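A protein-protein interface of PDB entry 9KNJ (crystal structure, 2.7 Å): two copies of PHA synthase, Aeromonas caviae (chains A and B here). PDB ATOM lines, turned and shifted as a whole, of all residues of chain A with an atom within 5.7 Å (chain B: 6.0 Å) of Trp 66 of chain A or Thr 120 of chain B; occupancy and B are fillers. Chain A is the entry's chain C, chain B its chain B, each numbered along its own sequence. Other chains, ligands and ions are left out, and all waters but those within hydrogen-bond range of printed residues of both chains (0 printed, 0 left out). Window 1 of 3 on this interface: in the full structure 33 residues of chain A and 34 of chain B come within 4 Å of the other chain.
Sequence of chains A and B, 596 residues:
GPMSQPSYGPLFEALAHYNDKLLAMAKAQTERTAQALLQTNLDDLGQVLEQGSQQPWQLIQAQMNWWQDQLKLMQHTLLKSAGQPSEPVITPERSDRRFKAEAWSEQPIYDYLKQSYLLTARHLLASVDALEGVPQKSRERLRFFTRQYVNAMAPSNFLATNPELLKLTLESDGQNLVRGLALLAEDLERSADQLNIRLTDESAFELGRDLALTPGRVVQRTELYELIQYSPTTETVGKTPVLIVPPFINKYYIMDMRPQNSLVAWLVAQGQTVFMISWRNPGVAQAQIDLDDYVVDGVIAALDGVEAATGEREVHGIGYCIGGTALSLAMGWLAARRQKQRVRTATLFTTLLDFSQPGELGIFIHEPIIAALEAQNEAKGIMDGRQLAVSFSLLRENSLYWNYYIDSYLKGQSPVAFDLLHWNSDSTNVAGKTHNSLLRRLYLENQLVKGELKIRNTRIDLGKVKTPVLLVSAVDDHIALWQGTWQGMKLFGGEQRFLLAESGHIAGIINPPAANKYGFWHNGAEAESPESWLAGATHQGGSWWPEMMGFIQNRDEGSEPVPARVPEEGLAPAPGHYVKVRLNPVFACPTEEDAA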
ATOM      1  N   GLN A  61       7.492  10.695  -0.533  1.00  0.00           N
ATOM      2  CA  GLN A  61       6.219  10.947  -1.203  1.00  0.00           C
ATOM      3  C   GLN A  61       6.159  12.362  -1.764  1.00  0.00           C
ATOM      4  O   GLN A  61       5.563  12.584  -2.823  1.00  0.00           O
ATOM      5  CB  GLN A  61       5.055  10.700  -0.240  1.00  0.00           C
ATOM      6  CG  GLN A  61       3.677  10.848  -0.879  1.00  0.00           C
ATOM      7  CD  GLN A  61       3.364   9.735  -1.867  1.00  0.00           C
ATOM      8  OE1 GLN A  61       3.048   8.610  -1.476  1.00  0.00           O
ATOM      9  NE2 GLN A  61       3.459  10.044  -3.155  1.00  0.00           N
ATOM     10  N   ALA A  62       6.774  13.328  -1.076  1.00  0.00           N
ATOM     11  CA  ALA A  62       6.817  14.690  -1.597  1.00  0.00           C
ATOM     12  C   ALA A  62       7.597  14.760  -2.908  1.00  0.00           C
ATOM     13  O   ALA A  62       7.209  15.487  -3.829  1.00  0.00           O
ATOM     14  CB  ALA A  62       7.422  15.634  -0.559  1.00  0.00           C
ATOM     15  N   GLN A  63       8.710  14.026  -3.005  1.00  0.00           N
ATOM     16  CA  GLN A  63       9.436  13.963  -4.270  1.00  0.00           C
ATOM     17  C   GLN A  63       8.587  13.318  -5.355  1.00  0.00           C
ATOM     18  O   GLN A  63       8.521  13.816  -6.485  1.00  0.00           O
ATOM     19  CB  GLN A  63      10.747  13.192  -4.102  1.00  0.00           C
ATOM     20  CG  GLN A  63      11.346  13.243  -2.708  1.00  0.00           C
ATOM     21  CD  GLN A  63      12.040  14.563  -2.415  1.00  0.00           C
ATOM     22  OE1 GLN A  63      12.182  15.414  -3.293  1.00  0.00           O
ATOM     23  NE2 GLN A  63      12.474  14.738  -1.172  1.00  0.00           N
ATOM     24  N   MET A  64       7.922  12.208  -5.025  1.00  0.00           N
ATOM     25  CA  MET A  64       7.111  11.507  -6.011  1.00  0.00           C
ATOM     26  C   MET A  64       5.915  12.339  -6.450  1.00  0.00           C
ATOM     27  O   MET A  64       5.477  12.225  -7.599  1.00  0.00           O
ATOM     28  CB  MET A  64       6.650  10.164  -5.450  1.00  0.00           C
ATOM     29  CG  MET A  64       7.733   9.093  -5.217  1.00  0.00           C
ATOM     30  SD  MET A  64       9.004   8.763  -6.478  1.00  0.00           S
ATOM     31  CE  MET A  64      10.161  10.138  -6.359  1.00  0.00           C
ATOM     32  N   ASN A  65       5.372  13.165  -5.552  1.00  0.00           N
ATOM     33  CA  ASN A  65       4.306  14.080  -5.944  1.00  0.00           C
ATOM     34  C   ASN A  65       4.798  15.082  -6.981  1.00  0.00           C
ATOM     35  O   ASN A  65       4.083  15.396  -7.941  1.00  0.00           O
ATOM     36  CB  ASN A  65       3.759  14.798  -4.712  1.00  0.00           C
ATOM     37  CG  ASN A  65       2.936  13.885  -3.838  1.00  0.00           C
ATOM     38  OD1 ASN A  65       2.746  12.713  -4.162  1.00  0.00           O
ATOM     39  ND2 ASN A  65       2.439  14.412  -2.725  1.00  0.00           N
ATOM     40  N   TRP A  66       6.020  15.593  -6.808  1.00  0.00           N
ATOM     41  CA  TRP A  66       6.566  16.535  -7.778  1.00  0.00           C
ATOM     42  C   TRP A  66       6.752  15.875  -9.142  1.00  0.00           C
ATOM     43  O   TRP A  66       6.346  16.428 -10.171  1.00  0.00           O
ATOM     44  CB  TRP A  66       7.891  17.112  -7.271  1.00  0.00           C
ATOM     45  CG  TRP A  66       8.425  18.216  -8.144  1.00  0.00           C
ATOM     46  CD1 TRP A  66       8.213  19.556  -7.992  1.00  0.00           C
ATOM     47  CD2 TRP A  66       9.247  18.072  -9.313  1.00  0.00           C
ATOM     48  NE1 TRP A  66       8.854  20.255  -8.989  1.00  0.00           N
ATOM     49  CE2 TRP A  66       9.495  19.366  -9.812  1.00  0.00           C
ATOM     50  CE3 TRP A  66       9.798  16.974  -9.984  1.00  0.00           C
ATOM     51  CZ2 TRP A  66      10.271  19.594 -10.951  1.00  0.00           C
ATOM     52  CZ3 TRP A  66      10.567  17.203 -11.116  1.00  0.00           C
ATOM     53  CH2 TRP A  66      10.794  18.502 -11.587  1.00  0.00           C
ATOM     54  N   TRP A  67       7.353  14.681  -9.167  1.00  0.00           N
ATOM     55  CA  TRP A  67       7.632  14.018 -10.439  1.00  0.00           C
ATOM     56  C   TRP A  67       6.349  13.700 -11.193  1.00  0.00           C
ATOM     57  O   TRP A  67       6.276  13.889 -12.413  1.00  0.00           O
ATOM     58  CB  TRP A  67       8.434  12.740 -10.206  1.00  0.00           C
ATOM     59  CG  TRP A  67       9.887  12.959  -9.930  1.00  0.00           C
ATOM     60  CD1 TRP A  67      10.473  13.128  -8.711  1.00  0.00           C
ATOM     61  CD2 TRP A  67      10.944  13.021 -10.895  1.00  0.00           C
ATOM     62  NE1 TRP A  67      11.828  13.295  -8.854  1.00  0.00           N
ATOM     63  CE2 TRP A  67      12.144  13.232 -10.186  1.00  0.00           C
ATOM     64  CE3 TRP A  67      10.992  12.921 -12.289  1.00  0.00           C
ATOM     65  CZ2 TRP A  67      13.379  13.346 -10.823  1.00  0.00           C
ATOM     66  CZ3 TRP A  67      12.220  13.032 -12.920  1.00  0.00           C
ATOM     67  CH2 TRP A  67      13.395  13.243 -12.187  1.00  0.00           C
ATOM     68  N   GLN A  68       5.328  13.210 -10.487  1.00  0.00           N
ATOM     69  CA  GLN A  68       4.075  12.867 -11.152  1.00  0.00           C
ATOM     70  C   GLN A  68       3.324  14.114 -11.609  1.00  0.00           C
ATOM     71  O   GLN A  68       2.807  14.153 -12.730  1.00  0.00           O
ATOM     72  CB  GLN A  68       3.203  12.021 -10.224  1.00  0.00           C
ATOM     73  CG  GLN A  68       2.251  11.076 -10.945  1.00  0.00           C
ATOM     74  CD  GLN A  68       0.931  10.900 -10.211  1.00  0.00           C
ATOM     75  OE1 GLN A  68       0.648  11.605  -9.239  1.00  0.00           O
ATOM     76  NE2 GLN A  68       0.118   9.955 -10.672  1.00  0.00           N
ATOM     77  N   ASP A  69       3.255  15.142 -10.762  1.00  0.00           N
ATOM     78  CA  ASP A  69       2.472  16.322 -11.114  1.00  0.00           C
ATOM     79  C   ASP A  69       3.145  17.132 -12.217  1.00  0.00           C
ATOM     80  O   ASP A  69       2.464  17.713 -13.070  1.00  0.00           O
ATOM     81  CB  ASP A  69       2.231  17.183  -9.875  1.00  0.00           C
ATOM     82  CG  ASP A  69       1.215  16.566  -8.934  1.00  0.00           C
ATOM     83  OD1 ASP A  69       0.589  15.555  -9.327  1.00  0.00           O
ATOM     84  OD2 ASP A  69       1.046  17.086  -7.807  1.00  0.00           O
ATOM     85  N   GLN A  70       4.478  17.193 -12.213  1.00  0.00           N
ATOM     86  CA  GLN A  70       5.172  17.880 -13.296  1.00  0.00           C
ATOM     87  C   GLN A  70       5.035  17.115 -14.608  1.00  0.00           C
ATOM     88  O   GLN A  70       4.886  17.723 -15.674  1.00  0.00           O
ATOM     89  CB  GLN A  70       6.642  18.086 -12.933  1.00  0.00           C
ATOM     90  CG  GLN A  70       7.394  18.975 -13.904  1.00  0.00           C
ATOM     91  CD  GLN A  70       7.146  20.446 -13.663  1.00  0.00           C
ATOM     92  OE1 GLN A  70       7.381  21.278 -14.539  1.00  0.00           O
ATOM     93  NE2 GLN A  70       6.670  20.777 -12.471  1.00  0.00           N
ATOM     94  N   LEU A  71       5.079  15.780 -14.549  1.00  0.00           N
ATOM     95  CA  LEU A  71       4.861  14.974 -15.748  1.00  0.00           C
ATOM     96  C   LEU A  71       3.420  15.083 -16.235  1.00  0.00           C
ATOM     97  O   LEU A  71       3.168  15.046 -17.443  1.00  0.00           O
ATOM     98  CB  LEU A  71       5.232  13.516 -15.474  1.00  0.00           C
ATOM     99  CG  LEU A  71       5.142  12.537 -16.648  1.00  0.00           C
ATOM    100  CD1 LEU A  71       6.033  12.976 -17.798  1.00  0.00           C
ATOM    101  CD2 LEU A  71       5.508  11.132 -16.196  1.00  0.00           C
ATOM    102  N   SER A 116       4.347  25.229 -12.947  1.00  0.00           N
ATOM    103  CA  SER A 116       5.470  24.431 -12.463  1.00  0.00           C
ATOM    104  C   SER A 116       6.101  25.056 -11.225  1.00  0.00           C
ATOM    105  O   SER A 116       6.644  24.340 -10.375  1.00  0.00           O
ATOM    106  CB  SER A 116       6.516  24.258 -13.566  1.00  0.00           C
ATOM    107  OG  SER A 116       6.588  25.407 -14.386  1.00  0.00           O
ATOM    108  N   LEU A 119       4.245  23.851  -8.308  1.00  0.00           N
ATOM    109  CA  LEU A 119       4.687  22.513  -7.936  1.00  0.00           C
ATOM    110  C   LEU A 119       5.992  22.554  -7.152  1.00  0.00           C
ATOM    111  O   LEU A 119       6.172  21.790  -6.198  1.00  0.00           O
ATOM    112  CB  LEU A 119       4.836  21.648  -9.183  1.00  0.00           C
ATOM    113  CG  LEU A 119       3.518  21.286  -9.862  1.00  0.00           C
ATOM    114  CD1 LEU A 119       3.760  20.351 -11.032  1.00  0.00           C
ATOM    115  CD2 LEU A 119       2.548  20.671  -8.862  1.00  0.00           C
ATOM    116  N   THR A 120       6.919  23.432  -7.548  1.00  0.00           N
ATOM    117  CA  THR A 120       8.155  23.594  -6.787  1.00  0.00           C
ATOM    118  C   THR A 120       7.870  24.110  -5.381  1.00  0.00           C
ATOM    119  O   THR A 120       8.453  23.625  -4.402  1.00  0.00           O
ATOM    120  CB  THR A 120       9.110  24.534  -7.530  1.00  0.00           C
ATOM    121  OG1 THR A 120       9.806  23.806  -8.551  1.00  0.00           O
ATOM    122  CG2 THR A 120      10.126  25.148  -6.577  1.00  0.00           C
ATOM    123  N   HIS A 123       6.372  21.314  -3.415  1.00  0.00           N
ATOM    124  CA  HIS A 123       7.430  20.378  -3.050  1.00  0.00           C
ATOM    125  C   HIS A 123       8.255  20.903  -1.878  1.00  0.00           C
ATOM    126  O   HIS A 123       8.611  20.139  -0.974  1.00  0.00           O
ATOM    127  CB  HIS A 123       8.313  20.105  -4.269  1.00  0.00           C
ATOM    128  CG  HIS A 123       9.597  19.405  -3.952  1.00  0.00           C
ATOM    129  ND1 HIS A 123      10.806  20.066  -3.881  1.00  0.00           N
ATOM    130  CD2 HIS A 123       9.866  18.101  -3.707  1.00  0.00           C
ATOM    131  CE1 HIS A 123      11.762  19.199  -3.596  1.00  0.00           C
ATOM    132  NE2 HIS A 123      11.219  18.001  -3.486  1.00  0.00           N
ATOM    133  N   TRP B  66      15.407  30.666  -9.963  1.00  0.00           N
ATOM    134  CA  TRP B  66      14.574  29.581 -10.471  1.00  0.00           C
ATOM    135  C   TRP B  66      13.804  30.006 -11.716  1.00  0.00           C
ATOM    136  O   TRP B  66      13.725  29.247 -12.688  1.00  0.00           O
ATOM    137  CB  TRP B  66      13.605  29.090  -9.395  1.00  0.00           C
ATOM    138  CG  TRP B  66      12.860  27.863  -9.837  1.00  0.00           C
ATOM    139  CD1 TRP B  66      13.224  26.570  -9.624  1.00  0.00           C
ATOM    140  CD2 TRP B  66      11.640  27.818 -10.594  1.00  0.00           C
ATOM    141  NE1 TRP B  66      12.306  25.719 -10.193  1.00  0.00           N
ATOM    142  CE2 TRP B  66      11.324  26.460 -10.793  1.00  0.00           C
ATOM    143  CE3 TRP B  66      10.784  28.793 -11.117  1.00  0.00           C
ATOM    144  CZ2 TRP B  66      10.190  26.051 -11.492  1.00  0.00           C
ATOM    145  CZ3 TRP B  66       9.656  28.384 -11.814  1.00  0.00           C
ATOM    146  CH2 TRP B  66       9.371  27.025 -11.993  1.00  0.00           C
ATOM    147  N   GLN B  70      14.785  28.181 -15.172  1.00  0.00           N
ATOM    148  CA  GLN B  70      13.763  27.335 -15.779  1.00  0.00           C
ATOM    149  C   GLN B  70      13.419  27.815 -17.182  1.00  0.00           C
ATOM    150  O   GLN B  70      13.347  27.009 -18.115  1.00  0.00           O
ATOM    151  CB  GLN B  70      12.515  27.287 -14.896  1.00  0.00           C
ATOM    152  CG  GLN B  70      11.466  26.279 -15.350  1.00  0.00           C
ATOM    153  CD  GLN B  70      11.801  24.853 -14.958  1.00  0.00           C
ATOM    154  OE1 GLN B  70      12.334  24.602 -13.879  1.00  0.00           O
ATOM    155  NE2 GLN B  70      11.485  23.910 -15.837  1.00  0.00           N
ATOM    156  N   LEU B 113      12.780  16.585 -17.559  1.00  0.00           N
ATOM    157  CA  LEU B 113      12.148  16.374 -16.260  1.00  0.00           C
ATOM    158  C   LEU B 113      13.185  16.239 -15.156  1.00  0.00           C
ATOM    159  O   LEU B 113      13.005  16.771 -14.054  1.00  0.00           O
ATOM    160  CB  LEU B 113      11.255  15.136 -16.301  1.00  0.00           C
ATOM    161  CG  LEU B 113       9.933  15.259 -15.549  1.00  0.00           C
ATOM    162  CD1 LEU B 113       9.427  16.687 -15.613  1.00  0.00           C
ATOM    163  CD2 LEU B 113       8.915  14.300 -16.123  1.00  0.00           C
ATOM    164  N   LYS B 114      14.271  15.512 -15.427  1.00  0.00           N
ATOM    165  CA  LYS B 114      15.373  15.446 -14.474  1.00  0.00           C
ATOM    166  C   LYS B 114      15.940  16.832 -14.206  1.00  0.00           C
ATOM    167  O   LYS B 114      16.083  17.241 -13.050  1.00  0.00           O
ATOM    168  CB  LYS B 114      16.465  14.510 -14.993  1.00  0.00           C
ATOM    169  CG  LYS B 114      17.407  14.004 -13.908  1.00  0.00           C
ATOM    170  CD  LYS B 114      17.575  12.493 -13.979  1.00  0.00           C
ATOM    171  CE  LYS B 114      17.960  11.911 -12.628  1.00  0.00           C
ATOM    172  NZ  LYS B 114      18.454  10.509 -12.747  1.00  0.00           N
ATOM    173  N   GLN B 115      16.238  17.585 -15.272  1.00  0.00           N
ATOM    174  CA  GLN B 115      16.885  18.885 -15.110  1.00  0.00           C
ATOM    175  C   GLN B 115      16.021  19.845 -14.299  1.00  0.00           C
ATOM    176  O   GLN B 115      16.531  20.550 -13.422  1.00  0.00           O
ATOM    177  CB  GLN B 115      17.213  19.485 -16.480  1.00  0.00           C
ATOM    178  CG  GLN B 115      18.382  18.828 -17.209  1.00  0.00           C
ATOM    179  CD  GLN B 115      19.675  18.857 -16.416  1.00  0.00           C
ATOM    180  OE1 GLN B 115      19.959  19.816 -15.702  1.00  0.00           O
ATOM    181  NE2 GLN B 115      20.469  17.801 -16.544  1.00  0.00           N
ATOM    182  N   SER B 116      14.713  19.884 -14.570  1.00  0.00           N
ATOM    183  CA  SER B 116      13.834  20.758 -13.799  1.00  0.00           C
ATOM    184  C   SER B 116      13.852  20.403 -12.320  1.00  0.00           C
ATOM    185  O   SER B 116      13.660  21.277 -11.467  1.00  0.00           O
ATOM    186  CB  SER B 116      12.406  20.686 -14.339  1.00  0.00           C
ATOM    187  OG  SER B 116      12.396  20.564 -15.748  1.00  0.00           O
ATOM    188  N   TYR B 117      14.081  19.130 -11.996  1.00  0.00           N
ATOM    189  CA  TYR B 117      14.158  18.725 -10.596  1.00  0.00           C
ATOM    190  C   TYR B 117      15.412  19.276  -9.926  1.00  0.00           C
ATOM    191  O   TYR B 117      15.367  19.678  -8.757  1.00  0.00           O
ATOM    192  CB  TYR B 117      14.112  17.202 -10.490  1.00  0.00           C
ATOM    193  CG  TYR B 117      13.989  16.698  -9.075  1.00  0.00           C
ATOM    194  CD1 TYR B 117      13.042  17.231  -8.210  1.00  0.00           C
ATOM    195  CD2 TYR B 117      14.824  15.697  -8.599  1.00  0.00           C
ATOM    196  CE1 TYR B 117      12.927  16.776  -6.910  1.00  0.00           C
ATOM    197  CE2 TYR B 117      14.719  15.237  -7.301  1.00  0.00           C
ATOM    198  CZ  TYR B 117      13.769  15.780  -6.459  1.00  0.00           C
ATOM    199  OH  TYR B 117      13.658  15.324  -5.166  1.00  0.00           O
ATOM    200  N   LEU B 118      16.546  19.298 -10.639  1.00  0.00           N
ATOM    201  CA  LEU B 118      17.748  19.901 -10.069  1.00  0.00           C
ATOM    202  C   LEU B 118      17.529  21.375  -9.761  1.00  0.00           C
ATOM    203  O   LEU B 118      18.067  21.899  -8.779  1.00  0.00           O
ATOM    204  CB  LEU B 118      18.953  19.736 -11.002  1.00  0.00           C
ATOM    205  CG  LEU B 118      19.605  18.363 -11.213  1.00  0.00           C
ATOM    206  CD1 LEU B 118      19.623  17.576  -9.905  1.00  0.00           C
ATOM    207  CD2 LEU B 118      19.003  17.556 -12.355  1.00  0.00           C
ATOM    208  N   LEU B 119      16.759  22.065 -10.601  1.00  0.00           N
ATOM    209  CA  LEU B 119      16.408  23.451 -10.316  1.00  0.00           C
ATOM    210  C   LEU B 119      15.534  23.555  -9.073  1.00  0.00           C
ATOM    211  O   LEU B 119      15.685  24.491  -8.280  1.00  0.00           O
ATOM    212  CB  LEU B 119      15.703  24.066 -11.523  1.00  0.00           C
ATOM    213  CG  LEU B 119      16.586  24.628 -12.637  1.00  0.00           C
ATOM    214  CD1 LEU B 119      17.274  23.536 -13.437  1.00  0.00           C
ATOM    215  CD2 LEU B 119      15.724  25.455 -13.546  1.00  0.00           C
ATOM    216  N   THR B 120      14.602  22.614  -8.896  1.00  0.00           N
ATOM    217  CA  THR B 120      13.769  22.615  -7.698  1.00  0.00           C
ATOM    218  C   THR B 120      14.598  22.337  -6.448  1.00  0.00           C
ATOM    219  O   THR B 120      14.367  22.945  -5.395  1.00  0.00           O
ATOM    220  CB  THR B 120      12.644  21.591  -7.838  1.00  0.00           C
ATOM    221  OG1 THR B 120      12.000  21.762  -9.105  1.00  0.00           O
ATOM    222  CG2 THR B 120      11.617  21.773  -6.736  1.00  0.00           C
ATOM    223  N   ALA B 121      15.560  21.414  -6.544  1.00  0.00           N
ATOM    224  CA  ALA B 121      16.448  21.147  -5.415  1.00  0.00           C
ATOM    225  C   ALA B 121      17.298  22.366  -5.084  1.00  0.00           C
ATOM    226  O   ALA B 121      17.471  22.710  -3.907  1.00  0.00           O
ATOM    227  CB  ALA B 121      17.336  19.940  -5.715  1.00  0.00           C
ATOM    228  N   ARG B 122      17.833  23.035  -6.110  1.00  0.00           N
ATOM    229  CA  ARG B 122      18.584  24.265  -5.881  1.00  0.00           C
ATOM    230  C   ARG B 122      17.709  25.326  -5.233  1.00  0.00           C
ATOM    231  O   ARG B 122      18.154  26.040  -4.326  1.00  0.00           O
ATOM    232  CB  ARG B 122      19.158  24.787  -7.198  1.00  0.00           C
ATOM    233  CG  ARG B 122      20.586  24.364  -7.457  1.00  0.00           C
ATOM    234  CD  ARG B 122      20.777  23.895  -8.892  1.00  0.00           C
ATOM    235  NE  ARG B 122      22.186  23.716  -9.223  1.00  0.00           N
ATOM    236  CZ  ARG B 122      23.016  24.703  -9.537  1.00  0.00           C
ATOM    237  NH1 ARG B 122      22.605  25.961  -9.591  1.00  0.00           N
ATOM    238  NH2 ARG B 122      24.288  24.421  -9.802  1.00  0.00           N
ATOM    239  N   HIS B 123      16.440  25.384  -5.629  1.00  0.00           N
ATOM    240  CA  HIS B 123      15.518  26.392  -5.045  1.00  0.00           C
ATOM    241  C   HIS B 123      15.357  26.110  -3.553  1.00  0.00           C
ATOM    242  O   HIS B 123      15.466  27.038  -2.736  1.00  0.00           O
ATOM    243  CB  HIS B 123      14.152  26.372  -5.735  1.00  0.00           C
ATOM    244  CG  HIS B 123      13.204  27.397  -5.214  1.00  0.00           C
ATOM    245  ND1 HIS B 123      12.057  27.069  -4.527  1.00  0.00           N
ATOM    246  CD2 HIS B 123      13.245  28.730  -5.254  1.00  0.00           C
ATOM    247  CE1 HIS B 123      11.425  28.180  -4.182  1.00  0.00           C
ATOM    248  NE2 HIS B 123      12.130  29.199  -4.614  1.00  0.00           N
ATOM    249  N   LEU B 124      15.088  24.852  -3.215  1.00  0.00           N
ATOM    250  CA  LEU B 124      14.884  24.488  -1.794  1.00  0.00           C
ATOM    251  C   LEU B 124      16.179  24.785  -1.044  1.00  0.00           C
ATOM    252  O   LEU B 124      16.111  25.414   0.019  1.00  0.00           O
ATOM    253  CB  LEU B 124      14.508  23.009  -1.713  1.00  0.00           C
ATOM    254  CG  LEU B 124      14.423  22.407  -0.312  1.00  0.00           C
ATOM    255  CD1 LEU B 124      13.580  23.276   0.601  1.00  0.00           C
ATOM    256  CD2 LEU B 124      13.837  21.008  -0.379  1.00  0.00           C
ATOM    257  N   LEU B 125      17.316  24.376  -1.602  1.00  0.00           N
ATOM    258  CA  LEU B 125      18.555  24.574  -0.857  1.00  0.00           C
ATOM    259  C   LEU B 125      18.845  26.054  -0.642  1.00  0.00           C
ATOM    260  O   LEU B 125      19.204  26.468   0.467  1.00  0.00           O
ATOM    261  CB  LEU B 125      19.718  23.902  -1.583  1.00  0.00           C
ATOM    262  CG  LEU B 125      20.164  22.584  -0.951  1.00  0.00           C
ATOM    263  CD1 LEU B 125      20.589  22.810   0.490  1.00  0.00           C
ATOM    264  CD2 LEU B 125      19.052  21.556  -1.023  1.00  0.00           C
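Leu 113 of chain B touches Trp 66 of chain A. Trp 66 of chain A touches Tyr 117 of chain B. O of Leu 113 of chain B touches CZ3 of Trp 67 of chain A, at 3.99 Å. Lys 114 of chain B touches Trp 67 of chain A (CA to CH2, 3.7 Å). Trp 67 of chain A touches Tyr 117 of chain B (CZ2 to CD2, 3.5 Å). Leu 113 of chain B touches Gln 70 of chain A. Trp 66 of chain B touches Ser 116 of chain A. Thr 120 of chain A touches Trp 66 of chain B (OG1 to NE1, 3.6 Å). His 123 of chain A touches Tyr 117 of chain B. ND1 of His 123 of chain A touches CG2 of Thr 120 of chain B, 3.4 Å away.
The side-chain hydroxyl (OG1) of Thr 120 of chain B is in hydrogen-bond range of the side-chain hydroxyl (OG1) of Thr 120 of chain A (3.0 Å). The side-chain hydroxyl (OH) of Tyr 117 of chain B sits close to the side-chain amide oxygen (OE1) of Gln 63 of chain A, 2.4 Å away. OG1 of Thr 120 of chain B sits close to NE1 of Trp 66 of chain A.
Of chain B, only Leu 113 (3.7 Å), Ser 116 (3.7 Å), Tyr 117 (3.4 Å) and Thr 120 (3.3 Å) come within 4 Å of Trp 66 of chain A. Of the printed residues of chain B, Gln 70 of chain A touches Leu 113. Printed residues of chain B within 4 Å of Thr 120 of chain A: Trp 66, Thr 120 and His 123. Of the printed residues of chain A, Leu 113 of chain B touches Trp 66 (3.7 Å), Trp 67 (3.99 Å), Gln 70 (3.5 Å) and Leu 71 (3.6 Å). Printed residues of chain A within 4 Å of Lys 114 of chain B: Trp 67. Printed residues of chain A within 4 Å of Tyr 117 of chain B: Gln 63 (2.4 Å), Trp 66 (3.4 Å), Trp 67 (3.5 Å) and His 123 (3.99 Å). Of chain A, only Trp 66, Thr 120 and His 123 come within 4 Å of Thr 120 of chain B. The nearest residue of chain A that does not touch Thr 120 of chain B is Leu 119 of chain A (5.5 Å). The nearest printed residue of chain B that does not touch His 123 of chain A is Leu 124 of chain B (4.2 Å).
Trp 66 of chain A touches Ser 116 of chain B, and with the chains exchanged Ser 116 of chain A touches Trp 66 of chain B. Trp 66 of chain A touches Thr 120 of chain B, and with the chains exchanged Thr 120 of chain A touches Trp 66 of chain B. Thr 120 of chain A touches its own counterpart, Thr 120 of chain B. Thr 120 of chain A touches His 123 of chain B, and with the chains exchanged His 123 of chain A touches Thr 120 of chain B. Positions printed for both chains: 66, 70, 116, 119, 120 and 123.
The side-chain hydroxyl of Thr 120 of chain B sits at hydrogen-bond distance from the backbone carbonyl oxygen of Ser 116 of chain B (2.9 Å). The side-chain amide oxygen (OE1) of Gln 63 of chain A lies within hydrogen-bond range of a ring nitrogen (NE2) of His 123 of chain A. The side-chain amide nitrogen of Gln 70 of chain B sits at hydrogen-bond distance from the side-chain hydroxyl of Ser 116 of chain B (3.5 Å).
Hydrophobic or aromatic side chains of chain B that line the printed part of chain A: Trp 66, Leu 113, Tyr 117 and His 123. Along chain B the printed residues that touch a printed residue of chain A span positions 66 to 123. Printed residues of chain A that touch a printed residue of chain B: Gln 63, Trp 66, Trp 67, Gln 70, Leu 71, Ser 116, Thr 120 and His 123. Among the printed residues, no Asp or Glu carboxylate lies within 4 Å of a Lys or Arg side-chain nitrogen of the other chain.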
